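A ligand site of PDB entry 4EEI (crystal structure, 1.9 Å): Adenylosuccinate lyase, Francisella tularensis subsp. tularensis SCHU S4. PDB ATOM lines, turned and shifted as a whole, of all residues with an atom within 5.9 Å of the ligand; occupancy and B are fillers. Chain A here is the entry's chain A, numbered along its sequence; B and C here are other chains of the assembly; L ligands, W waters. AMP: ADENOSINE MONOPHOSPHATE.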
ATOM      1  N   GLU A  62      20.281  27.478   1.965  1.00  0.00           N
ATOM      2  CA  GLU A  62      19.034  26.728   1.854  1.00  0.00           C
ATOM      3  C   GLU A  62      18.668  26.001   3.147  1.00  0.00           C
ATOM      4  O   GLU A  62      17.489  25.676   3.378  1.00  0.00           O
ATOM      5  CB  GLU A  62      19.105  25.748   0.682  1.00  0.00           C
ATOM      6  CG  GLU A  62      17.748  25.134   0.340  1.00  0.00           C
ATOM      7  CD  GLU A  62      17.790  24.195  -0.866  1.00  0.00           C
ATOM      8  OE1 GLU A  62      18.830  24.138  -1.565  1.00  0.00           O
ATOM      9  OE2 GLU A  62      16.774  23.517  -1.122  1.00  0.00           O
ATOM     10  N   THR A  65      16.781  28.981   4.674  1.00  0.00           N
ATOM     11  CA  THR A  65      15.634  29.440   3.880  1.00  0.00           C
ATOM     12  C   THR A  65      14.623  28.345   3.574  1.00  0.00           C
ATOM     13  O   THR A  65      13.432  28.638   3.421  1.00  0.00           O
ATOM     14  CB  THR A  65      16.054  30.067   2.547  1.00  0.00           C
ATOM     15  OG1 THR A  65      16.578  29.041   1.690  1.00  0.00           O
ATOM     16  CG2 THR A  65      17.101  31.143   2.777  1.00  0.00           C
ATOM     17  N   LYS A  66      15.090  27.107   3.465  1.00  0.00           N
ATOM     18  CA  LYS A  66      14.271  25.973   3.018  1.00  0.00           C
ATOM     19  C   LYS A  66      13.703  26.226   1.628  1.00  0.00           C
ATOM     20  O   LYS A  66      12.659  25.671   1.277  1.00  0.00           O
ATOM     21  CB  LYS A  66      13.133  25.671   3.999  1.00  0.00           C
ATOM     22  CG  LYS A  66      13.565  25.502   5.454  1.00  0.00           C
ATOM     23  CD  LYS A  66      14.432  24.275   5.637  1.00  0.00           C
ATOM     24  CE  LYS A  66      14.728  24.064   7.124  1.00  0.00           C
ATOM     25  NZ  LYS A  66      15.781  23.021   7.342  1.00  0.00           N
ATOM     26  N   HIS A  67      14.381  27.048   0.843  1.00  0.00           N
ATOM     27  CA  HIS A  67      13.917  27.427  -0.487  1.00  0.00           C
ATOM     28  C   HIS A  67      15.137  27.632  -1.365  1.00  0.00           C
ATOM     29  O   HIS A  67      15.889  28.577  -1.164  1.00  0.00           O
ATOM     30  CB  HIS A  67      13.124  28.722  -0.384  1.00  0.00           C
ATOM     31  CG  HIS A  67      12.353  29.076  -1.620  1.00  0.00           C
ATOM     32  ND1 HIS A  67      12.946  29.212  -2.853  1.00  0.00           N
ATOM     33  CD2 HIS A  67      11.037  29.337  -1.804  1.00  0.00           C
ATOM     34  CE1 HIS A  67      12.032  29.526  -3.751  1.00  0.00           C
ATOM     35  NE2 HIS A  67      10.866  29.602  -3.142  1.00  0.00           N
ATOM     36  N   ASP A  68      15.344  26.746  -2.343  1.00  0.00           N
ATOM     37  CA  ASP A  68      16.578  26.752  -3.126  1.00  0.00           C
ATOM     38  C   ASP A  68      16.777  28.019  -3.972  1.00  0.00           C
ATOM     39  O   ASP A  68      17.900  28.476  -4.136  1.00  0.00           O
ATOM     40  CB  ASP A  68      16.716  25.466  -3.964  1.00  0.00           C
ATOM     41  CG  ASP A  68      15.564  25.237  -4.941  1.00  0.00           C
ATOM     42  OD1 ASP A  68      14.449  25.762  -4.710  1.00  0.00           O
ATOM     43  OD2 ASP A  68      15.775  24.523  -5.943  1.00  0.00           O
ATOM     44  N   ILE A  69      15.695  28.596  -4.486  1.00  0.00           N
ATOM     45  CA  ILE A  69      15.840  29.765  -5.353  1.00  0.00           C
ATOM     46  C   ILE A  69      16.142  31.027  -4.553  1.00  0.00           C
ATOM     47  O   ILE A  69      16.945  31.873  -4.963  1.00  0.00           O
ATOM     48  CB  ILE A  69      14.583  29.969  -6.233  1.00  0.00           C
ATOM     49  CG1 ILE A  69      14.223  28.666  -6.927  1.00  0.00           C
ATOM     50  CG2 ILE A  69      14.826  31.064  -7.253  1.00  0.00           C
ATOM     51  CD1 ILE A  69      15.417  28.003  -7.642  1.00  0.00           C
ATOM     52  N   THR A  93       8.556  35.338 -10.627  1.00  0.00           N
ATOM     53  CA  THR A  93       8.371  34.314  -9.606  1.00  0.00           C
ATOM     54  C   THR A  93       9.531  33.342  -9.742  1.00  0.00           C
ATOM     55  O   THR A  93      10.226  33.350 -10.766  1.00  0.00           O
ATOM     56  CB  THR A  93       7.005  33.608  -9.757  1.00  0.00           C
ATOM     57  OG1 THR A  93       6.792  32.749  -8.640  1.00  0.00           O
ATOM     58  CG2 THR A  93       6.954  32.798 -11.051  1.00  0.00           C
ATOM     59  N   SER A  94       9.790  32.518  -8.729  1.00  0.00           N
ATOM     60  CA  SER A  94      10.946  31.621  -8.776  1.00  0.00           C
ATOM     61  C   SER A  94      10.944  30.718 -10.003  1.00  0.00           C
ATOM     62  O   SER A  94      11.989  30.482 -10.610  1.00  0.00           O
ATOM     63  CB  SER A  94      11.020  30.759  -7.520  1.00  0.00           C
ATOM     64  OG  SER A  94      11.397  31.551  -6.408  1.00  0.00           O
ATOM     65  N   SER A  95       9.774  30.225 -10.380  1.00  0.00           N
ATOM     66  CA  SER A  95       9.712  29.304 -11.509  1.00  0.00           C
ATOM     67  C   SER A  95       9.862  29.970 -12.885  1.00  0.00           C
ATOM     68  O   SER A  95      10.152  29.285 -13.863  1.00  0.00           O
ATOM     69  CB  SER A  95       8.466  28.421 -11.436  1.00  0.00           C
ATOM     70  OG  SER A  95       8.621  27.479 -10.383  1.00  0.00           O
ATOM     71  N   ILE A  98      13.501  29.256 -12.789  1.00  0.00           N
ATOM     72  CA  ILE A  98      13.790  27.826 -12.864  1.00  0.00           C
ATOM     73  C   ILE A  98      13.462  27.216 -14.225  1.00  0.00           C
ATOM     74  O   ILE A  98      14.307  26.522 -14.818  1.00  0.00           O
ATOM     75  CB  ILE A  98      12.964  27.019 -11.835  1.00  0.00           C
ATOM     76  CG1 ILE A  98      13.331  27.402 -10.409  1.00  0.00           C
ATOM     77  CG2 ILE A  98      13.186  25.524 -12.044  1.00  0.00           C
ATOM     78  CD1 ILE A  98      12.341  26.851  -9.388  1.00  0.00           C
ATOM     79  N   GLN A 212       2.337  29.692 -13.061  1.00  0.00           N
ATOM     80  CA  GLN A 212       3.547  29.939 -12.293  1.00  0.00           C
ATOM     81  C   GLN A 212       4.679  29.208 -13.044  1.00  0.00           C
ATOM     82  O   GLN A 212       5.831  29.667 -13.064  1.00  0.00           O
ATOM     83  CB  GLN A 212       3.433  29.442 -10.857  1.00  0.00           C
ATOM     84  CG  GLN A 212       4.690  29.692 -10.035  1.00  0.00           C
ATOM     85  CD  GLN A 212       4.426  29.621  -8.538  1.00  0.00           C
ATOM     86  OE1 GLN A 212       4.697  28.606  -7.902  1.00  0.00           O
ATOM     87  NE2 GLN A 212       3.909  30.709  -7.978  1.00  0.00           N
ATOM     88  N   ARG A 301       0.039  25.602 -10.487  1.00  0.00           N
ATOM     89  CA  ARG A 301       1.265  24.829 -10.294  1.00  0.00           C
ATOM     90  C   ARG A 301       1.344  24.126  -8.952  1.00  0.00           C
ATOM     91  O   ARG A 301       0.836  24.610  -7.943  1.00  0.00           O
ATOM     92  CB  ARG A 301       2.506  25.707 -10.502  1.00  0.00           C
ATOM     93  CG  ARG A 301       3.079  26.304  -9.228  1.00  0.00           C
ATOM     94  CD  ARG A 301       3.775  25.263  -8.365  1.00  0.00           C
ATOM     95  NE  ARG A 301       4.921  24.641  -9.024  1.00  0.00           N
ATOM     96  CZ  ARG A 301       6.099  25.236  -9.197  1.00  0.00           C
ATOM     97  NH1 ARG A 301       6.293  26.476  -8.766  1.00  0.00           N
ATOM     98  NH2 ARG A 301       7.084  24.599  -9.811  1.00  0.00           N
ATOM     99  N   ILE A 303       4.574  21.550  -7.070  1.00  0.00           N
ATOM    100  CA  ILE A 303       6.003  21.312  -7.251  1.00  0.00           C
ATOM    101  C   ILE A 303       6.394  19.835  -7.354  1.00  0.00           C
ATOM    102  O   ILE A 303       7.571  19.504  -7.326  1.00  0.00           O
ATOM    103  CB  ILE A 303       6.826  22.003  -6.139  1.00  0.00           C
ATOM    104  CG1 ILE A 303       8.226  22.350  -6.659  1.00  0.00           C
ATOM    105  CG2 ILE A 303       6.904  21.136  -4.896  1.00  0.00           C
ATOM    106  CD1 ILE A 303       8.722  23.702  -6.214  1.00  0.00           C
ATOM    107  N   SER A 306       9.038  18.521  -9.603  1.00  0.00           N
ATOM    108  CA  SER A 306      10.397  18.999  -9.393  1.00  0.00           C
ATOM    109  C   SER A 306      11.341  17.887  -8.949  1.00  0.00           C
ATOM    110  O   SER A 306      12.375  17.673  -9.576  1.00  0.00           O
ATOM    111  CB  SER A 306      10.427  20.159  -8.410  1.00  0.00           C
ATOM    112  OG  SER A 306      11.763  20.528  -8.080  1.00  0.00           O
ATOM    113  N   SER A 307      10.984  17.171  -7.895  1.00  0.00           N
ATOM    114  CA  SER A 307      11.875  16.127  -7.392  1.00  0.00           C
ATOM    115  C   SER A 307      12.056  15.031  -8.436  1.00  0.00           C
ATOM    116  O   SER A 307      13.153  14.485  -8.586  1.00  0.00           O
ATOM    117  CB  SER A 307      11.328  15.540  -6.094  1.00  0.00           C
ATOM    118  OG  SER A 307      10.042  15.007  -6.306  1.00  0.00           O
ATOM    119  N   ARG A 310      14.436  16.147 -11.115  1.00  0.00           N
ATOM    120  CA  ARG A 310      15.814  16.184 -10.632  1.00  0.00           C
ATOM    121  C   ARG A 310      16.505  14.842 -10.840  1.00  0.00           C
ATOM    122  O   ARG A 310      17.717  14.783 -11.043  1.00  0.00           O
ATOM    123  CB  ARG A 310      15.891  16.566  -9.147  1.00  0.00           C
ATOM    124  CG  ARG A 310      15.554  18.018  -8.819  1.00  0.00           C
ATOM    125  CD  ARG A 310      15.732  18.231  -7.315  1.00  0.00           C
ATOM    126  NE  ARG A 310      15.050  19.411  -6.799  1.00  0.00           N
ATOM    127  CZ  ARG A 310      15.612  20.609  -6.686  1.00  0.00           C
ATOM    128  NH1 ARG A 310      16.873  20.805  -7.078  1.00  0.00           N
ATOM    129  NH2 ARG A 310      14.904  21.611  -6.191  1.00  0.00           N
ATOM    130  N   ARG B   4      20.968  15.832  -3.145  1.00  0.00           N
ATOM    131  CA  ARG B   4      19.834  16.462  -2.469  1.00  0.00           C
ATOM    132  C   ARG B   4      18.978  15.479  -1.653  1.00  0.00           C
ATOM    133  O   ARG B   4      18.494  15.834  -0.573  1.00  0.00           O
ATOM    134  CB  ARG B   4      18.961  17.205  -3.496  1.00  0.00           C
ATOM    135  CG  ARG B   4      17.771  17.966  -2.912  1.00  0.00           C
ATOM    136  CD  ARG B   4      17.091  18.813  -4.006  1.00  0.00           C
ATOM    137  NE  ARG B   4      16.055  19.689  -3.467  1.00  0.00           N
ATOM    138  CZ  ARG B   4      16.271  20.895  -2.960  1.00  0.00           C
ATOM    139  NH1 ARG B   4      17.502  21.394  -2.921  1.00  0.00           N
ATOM    140  NH2 ARG B   4      15.254  21.616  -2.492  1.00  0.00           N
ATOM    141  N   TYR B   5      18.825  14.246  -2.128  1.00  0.00           N
ATOM    142  CA  TYR B   5      17.979  13.262  -1.459  1.00  0.00           C
ATOM    143  C   TYR B   5      18.739  12.028  -0.963  1.00  0.00           C
ATOM    144  O   TYR B   5      18.141  11.025  -0.614  1.00  0.00           O
ATOM    145  CB  TYR B   5      16.858  12.795  -2.400  1.00  0.00           C
ATOM    146  CG  TYR B   5      16.090  13.924  -3.059  1.00  0.00           C
ATOM    147  CD1 TYR B   5      15.435  14.881  -2.300  1.00  0.00           C
ATOM    148  CD2 TYR B   5      16.026  14.014  -4.438  1.00  0.00           C
ATOM    149  CE1 TYR B   5      14.723  15.920  -2.898  1.00  0.00           C
ATOM    150  CE2 TYR B   5      15.308  15.039  -5.048  1.00  0.00           C
ATOM    151  CZ  TYR B   5      14.675  15.993  -4.281  1.00  0.00           C
ATOM    152  OH  TYR B   5      13.971  17.014  -4.893  1.00  0.00           O
ATOM    153  N   ASN B 270       2.717  26.041   3.034  1.00  0.00           N
ATOM    154  CA  ASN B 270       2.529  25.253   1.828  1.00  0.00           C
ATOM    155  C   ASN B 270       2.683  23.762   2.093  1.00  0.00           C
ATOM    156  O   ASN B 270       3.549  23.365   2.871  1.00  0.00           O
ATOM    157  CB  ASN B 270       3.512  25.688   0.737  1.00  0.00           C
ATOM    158  CG  ASN B 270       3.275  27.100   0.250  1.00  0.00           C
ATOM    159  OD1 ASN B 270       2.183  27.451  -0.176  1.00  0.00           O
ATOM    160  ND2 ASN B 270       4.310  27.930   0.321  1.00  0.00           N
ATOM    161  N   ILE B 272       4.678  21.721   0.747  1.00  0.00           N
ATOM    162  CA  ILE B 272       5.818  21.413  -0.094  1.00  0.00           C
ATOM    163  C   ILE B 272       6.356  20.009   0.128  1.00  0.00           C
ATOM    164  O   ILE B 272       6.887  19.388  -0.799  1.00  0.00           O
ATOM    165  CB  ILE B 272       6.964  22.425   0.066  1.00  0.00           C
ATOM    166  CG1 ILE B 272       7.301  22.604   1.549  1.00  0.00           C
ATOM    167  CG2 ILE B 272       6.583  23.762  -0.600  1.00  0.00           C
ATOM    168  CD1 ILE B 272       8.545  23.431   1.797  1.00  0.00           C
ATOM    169  N   GLU B 275       4.092  17.420  -1.615  1.00  0.00           N
ATOM    170  CA  GLU B 275       4.279  17.563  -3.061  1.00  0.00           C
ATOM    171  C   GLU B 275       5.569  16.872  -3.503  1.00  0.00           C
ATOM    172  O   GLU B 275       5.580  16.091  -4.462  1.00  0.00           O
ATOM    173  CB  GLU B 275       4.232  19.041  -3.491  1.00  0.00           C
ATOM    174  CG  GLU B 275       2.815  19.606  -3.434  1.00  0.00           C
ATOM    175  CD  GLU B 275       2.716  21.080  -3.754  1.00  0.00           C
ATOM    176  OE1 GLU B 275       3.689  21.662  -4.309  1.00  0.00           O
ATOM    177  OE2 GLU B 275       1.648  21.667  -3.475  1.00  0.00           O
ATOM    178  N   ASN B 276       6.643  17.130  -2.778  1.00  0.00           N
ATOM    179  CA  ASN B 276       7.894  16.399  -2.981  1.00  0.00           C
ATOM    180  C   ASN B 276       7.685  14.879  -2.972  1.00  0.00           C
ATOM    181  O   ASN B 276       8.196  14.167  -3.848  1.00  0.00           O
ATOM    182  CB  ASN B 276       8.935  16.787  -1.911  1.00  0.00           C
ATOM    183  CG  ASN B 276      10.235  16.006  -2.031  1.00  0.00           C
ATOM    184  OD1 ASN B 276      10.347  14.891  -1.523  1.00  0.00           O
ATOM    185  ND2 ASN B 276      11.233  16.582  -2.718  1.00  0.00           N
ATOM    186  N   TYR B 322      14.235   7.516   1.882  1.00  0.00           N
ATOM    187  CA  TYR B 322      14.052   8.969   1.978  1.00  0.00           C
ATOM    188  C   TYR B 322      12.584   9.340   2.136  1.00  0.00           C
ATOM    189  O   TYR B 322      12.236  10.159   2.988  1.00  0.00           O
ATOM    190  CB  TYR B 322      14.616   9.670   0.731  1.00  0.00           C
ATOM    191  CG  TYR B 322      14.386  11.182   0.732  1.00  0.00           C
ATOM    192  CD1 TYR B 322      15.316  12.035   1.290  1.00  0.00           C
ATOM    193  CD2 TYR B 322      13.245  11.738   0.158  1.00  0.00           C
ATOM    194  CE1 TYR B 322      15.120  13.406   1.308  1.00  0.00           C
ATOM    195  CE2 TYR B 322      13.030  13.120   0.174  1.00  0.00           C
ATOM    196  CZ  TYR B 322      13.981  13.940   0.743  1.00  0.00           C
ATOM    197  OH  TYR B 322      13.801  15.306   0.777  1.00  0.00           O
ATOM    198  N   ARG B 326      10.729  11.031   5.427  1.00  0.00           N
ATOM    199  CA  ARG B 326      10.222  12.402   5.292  1.00  0.00           C
ATOM    200  C   ARG B 326       8.715  12.445   5.542  1.00  0.00           C
ATOM    201  O   ARG B 326       8.205  13.361   6.200  1.00  0.00           O
ATOM    202  CB  ARG B 326      10.551  12.992   3.918  1.00  0.00           C
ATOM    203  CG  ARG B 326       9.974  14.385   3.710  1.00  0.00           C
ATOM    204  CD  ARG B 326      10.559  15.107   2.510  1.00  0.00           C
ATOM    205  NE  ARG B 326      10.104  16.506   2.477  1.00  0.00           N
ATOM    206  CZ  ARG B 326      10.615  17.443   1.687  1.00  0.00           C
ATOM    207  NH1 ARG B 326      11.600  17.134   0.856  1.00  0.00           N
ATOM    208  NH2 ARG B 326      10.148  18.680   1.749  1.00  0.00           N
ATOM    209  N   SER C 140      -1.024  28.461  -5.978  1.00  0.00           N
ATOM    210  CA  SER C 140       0.203  27.664  -6.109  1.00  0.00           C
ATOM    211  C   SER C 140       0.318  26.757  -4.885  1.00  0.00           C
ATOM    212  O   SER C 140       0.171  27.230  -3.764  1.00  0.00           O
ATOM    213  CB  SER C 140       1.425  28.573  -6.201  1.00  0.00           C
ATOM    214  OG  SER C 140       2.631  27.821  -6.086  1.00  0.00           O
ATOM    215  N   HIS C 141       0.550  25.458  -5.116  1.00  0.00           N
ATOM    216  CA  HIS C 141       0.527  24.470  -4.020  1.00  0.00           C
ATOM    217  C   HIS C 141      -0.868  24.418  -3.394  1.00  0.00           C
ATOM    218  O   HIS C 141      -1.018  24.008  -2.248  1.00  0.00           O
ATOM    219  CB  HIS C 141       1.552  24.762  -2.913  1.00  0.00           C
ATOM    220  CG  HIS C 141       2.905  25.137  -3.396  1.00  0.00           C
ATOM    221  ND1 HIS C 141       3.770  24.227  -3.973  1.00  0.00           N
ATOM    222  CD2 HIS C 141       3.577  26.312  -3.355  1.00  0.00           C
ATOM    223  CE1 HIS C 141       4.913  24.837  -4.275  1.00  0.00           C
ATOM    224  NE2 HIS C 141       4.815  26.098  -3.905  1.00  0.00           N
HETATM  225  P   AMP L   1      12.206  19.672  -4.172  1.00  0.00           P
HETATM  226  O1P AMP L   1      13.257  18.883  -3.431  1.00  0.00           O
HETATM  227  O2P AMP L   1      10.795  19.243  -3.887  1.00  0.00           O
HETATM  228  O3P AMP L   1      12.516  19.880  -5.624  1.00  0.00           O
HETATM  229  O5' AMP L   1      12.306  21.147  -3.520  1.00  0.00           O
HETATM  230  C5' AMP L   1      11.564  22.230  -4.058  1.00  0.00           C
HETATM  231  C4' AMP L   1      12.153  23.536  -3.540  1.00  0.00           C
HETATM  232  O4' AMP L   1      11.468  24.659  -4.120  1.00  0.00           O
HETATM  233  C3' AMP L   1      11.998  23.649  -2.035  1.00  0.00           C
HETATM  234  O3' AMP L   1      13.222  24.117  -1.479  1.00  0.00           O
HETATM  235  C2' AMP L   1      10.922  24.698  -1.835  1.00  0.00           C
HETATM  236  O2' AMP L   1      11.173  25.461  -0.661  1.00  0.00           O
HETATM  237  C1' AMP L   1      11.038  25.545  -3.083  1.00  0.00           C
HETATM  238  N9  AMP L   1       9.742  26.175  -3.429  1.00  0.00           N
HETATM  239  C8  AMP L   1       8.668  26.278  -2.640  1.00  0.00           C
HETATM  240  N7  AMP L   1       7.648  26.922  -3.276  1.00  0.00           N
HETATM  241  C5  AMP L   1       8.085  27.254  -4.502  1.00  0.00           C
HETATM  242  C6  AMP L   1       7.533  27.945  -5.684  1.00  0.00           C
HETATM  243  N6  AMP L   1       6.262  28.426  -5.681  1.00  0.00           N
HETATM  244  N1  AMP L   1       8.330  28.071  -6.765  1.00  0.00           N
HETATM  245  C2  AMP L   1       9.585  27.596  -6.784  1.00  0.00           C
HETATM  246  N3  AMP L   1      10.155  26.958  -5.749  1.00  0.00           N
HETATM  247  C4  AMP L   1       9.470  26.753  -4.601  1.00  0.00           C
HETATM  248  O   HOH W   1      13.159  19.066  -0.886  1.00  0.00           O
HETATM  249  O   HOH W   2       4.932  29.739  -3.226  1.00  0.00           O
HETATM  250  O   HOH W   3       9.362  20.507  -2.028  1.00  0.00           O
HETATM  251  O   HOH W   4       9.128  17.906  -5.754  1.00  0.00           O
HETATM  252  O   HOH W   5       7.590  30.099  -8.722  1.00  0.00           O
HETATM  253  O   HOH W   6      14.855  22.979   0.740  1.00  0.00           O
HETATM  254  O   HOH W   7      12.482  25.186  -6.495  1.00  0.00           O
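O of Lys 66 is in hydrogen-bond range of O2' of the ligand (2.5 Å).
An oxygen (O1P) of the ligand sits at hydrogen-bond distance from the side-chain hydroxyl of Tyr 5 of chain B (2.5 Å).
OG of Ser 306 sits at hydrogen-bond distance from O3P of the ligand (2.6 Å).
The side-chain amide oxygen of Gln 212 is in hydrogen-bond range of a nitrogen (N6) of the ligand (2.7 Å).
NE of Arg 310 is in salt-bridge range of O3P of the ligand (2.8 Å).
The guanidinium group (NE) of Arg 4 of chain B lies within salt-bridge range of an oxygen (O1P) of the ligand (2.9 Å).
The side-chain amide nitrogen (ND2) of Asn 276 of chain B is in hydrogen-bond range of an oxygen (O2P) of the ligand (2.9 Å).
A ring nitrogen (NE2) of His 141 of chain C sits at hydrogen-bond distance from a nitrogen (N7) of the ligand.
O3' of the ligand sits at hydrogen-bond distance from N of Asp 68.
The guanidinium group (NH1) of Arg 301 is in hydrogen-bond range of a nitrogen (N1) of the ligand.
OH of Tyr 5 of chain B lies close to NE of Arg 310.
The side-chain amide oxygen (OE1) of Gln 212 lies within hydrogen-bond range of the guanidinium group (NH1) of Arg 301.
The side-chain amide oxygen of Gln 212 lies within hydrogen-bond range of the side-chain hydroxyl of Ser 140 of chain C, at 2.9 Å.
OE2 of Glu 62 is in salt-bridge range of NH2 of Arg 4 of chain B, at 2.8 Å.
OG of Ser 307 lies within hydrogen-bond range of O of Asn 276 of chain B (3.2 Å).
The backbone carbonyl oxygen of Arg 301 sits at hydrogen-bond distance from the backbone NH of His 141 of chain C, at 3.0 Å.
The side-chain carboxylate of Glu 275 of chain B sits at hydrogen-bond distance from a ring nitrogen (ND1) of His 141 of chain C.
OE1 of Glu 275 of chain B sits at hydrogen-bond distance from N of Ile 303 (2.9 Å).
Glu 62 touches the ligand (OE2 to O3', 3.6 Å).
His 67 touches the ligand (CA to O2', 3.4 Å).
Ser 94 touches the ligand.
Ser 95 touches the ligand.
Ile 98 touches the ligand (CD1 to C2, 3.9 Å).
CD1 of Ile 303 touches C4 of the ligand, at 3.5 Å.
Ser 307 touches the ligand (N to O3P, 3.9 Å).
Ile 272 of chain B touches the ligand (CG2 to C8, 3.9 Å).
Ser 140 of chain C touches the ligand (OG to N6, 3.7 Å).
Hydrophobic or aromatic side chains that line the ligand: His 67, Ile 98, Ile 303, Tyr 5 of chain B, Ile 272 of chain B and His 141 of chain C.
The nearest printed residue that does not touch the ligand is Ile 69 (4.6 Å).
Water W1 bridges O1P of the ligand and NH1 of Arg 326 of chain B.
Water W7 bridges an oxygen (O4') of the ligand and the side-chain carboxylate (OD1) of Asp 68.
Water W3 lies within hydrogen-bond range of an oxygen (O2P) of the ligand and the backbone carbonyl oxygen of Ile 272 of chain B.
Water W4 lies within hydrogen-bond range of the backbone carbonyl oxygen of Ile 303 (2.7 Å), an oxygen (O2P) of the ligand (2.8 Å) and the backbone NH of Ser 307 (2.9 Å).
Water W5 lies within hydrogen-bond range of the backbone NH of Ser 95 (2.7 Å), the side-chain hydroxyl of Thr 93 (2.8 Å), a nitrogen (N1) of the ligand (2.9 Å), the backbone NH of Ser 94 (3.3 Å) and the side-chain amide oxygen of Gln 212 (3.4 Å).
Water W6 lies within hydrogen-bond range of OE2 of Glu 62 and O3' of the ligand.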
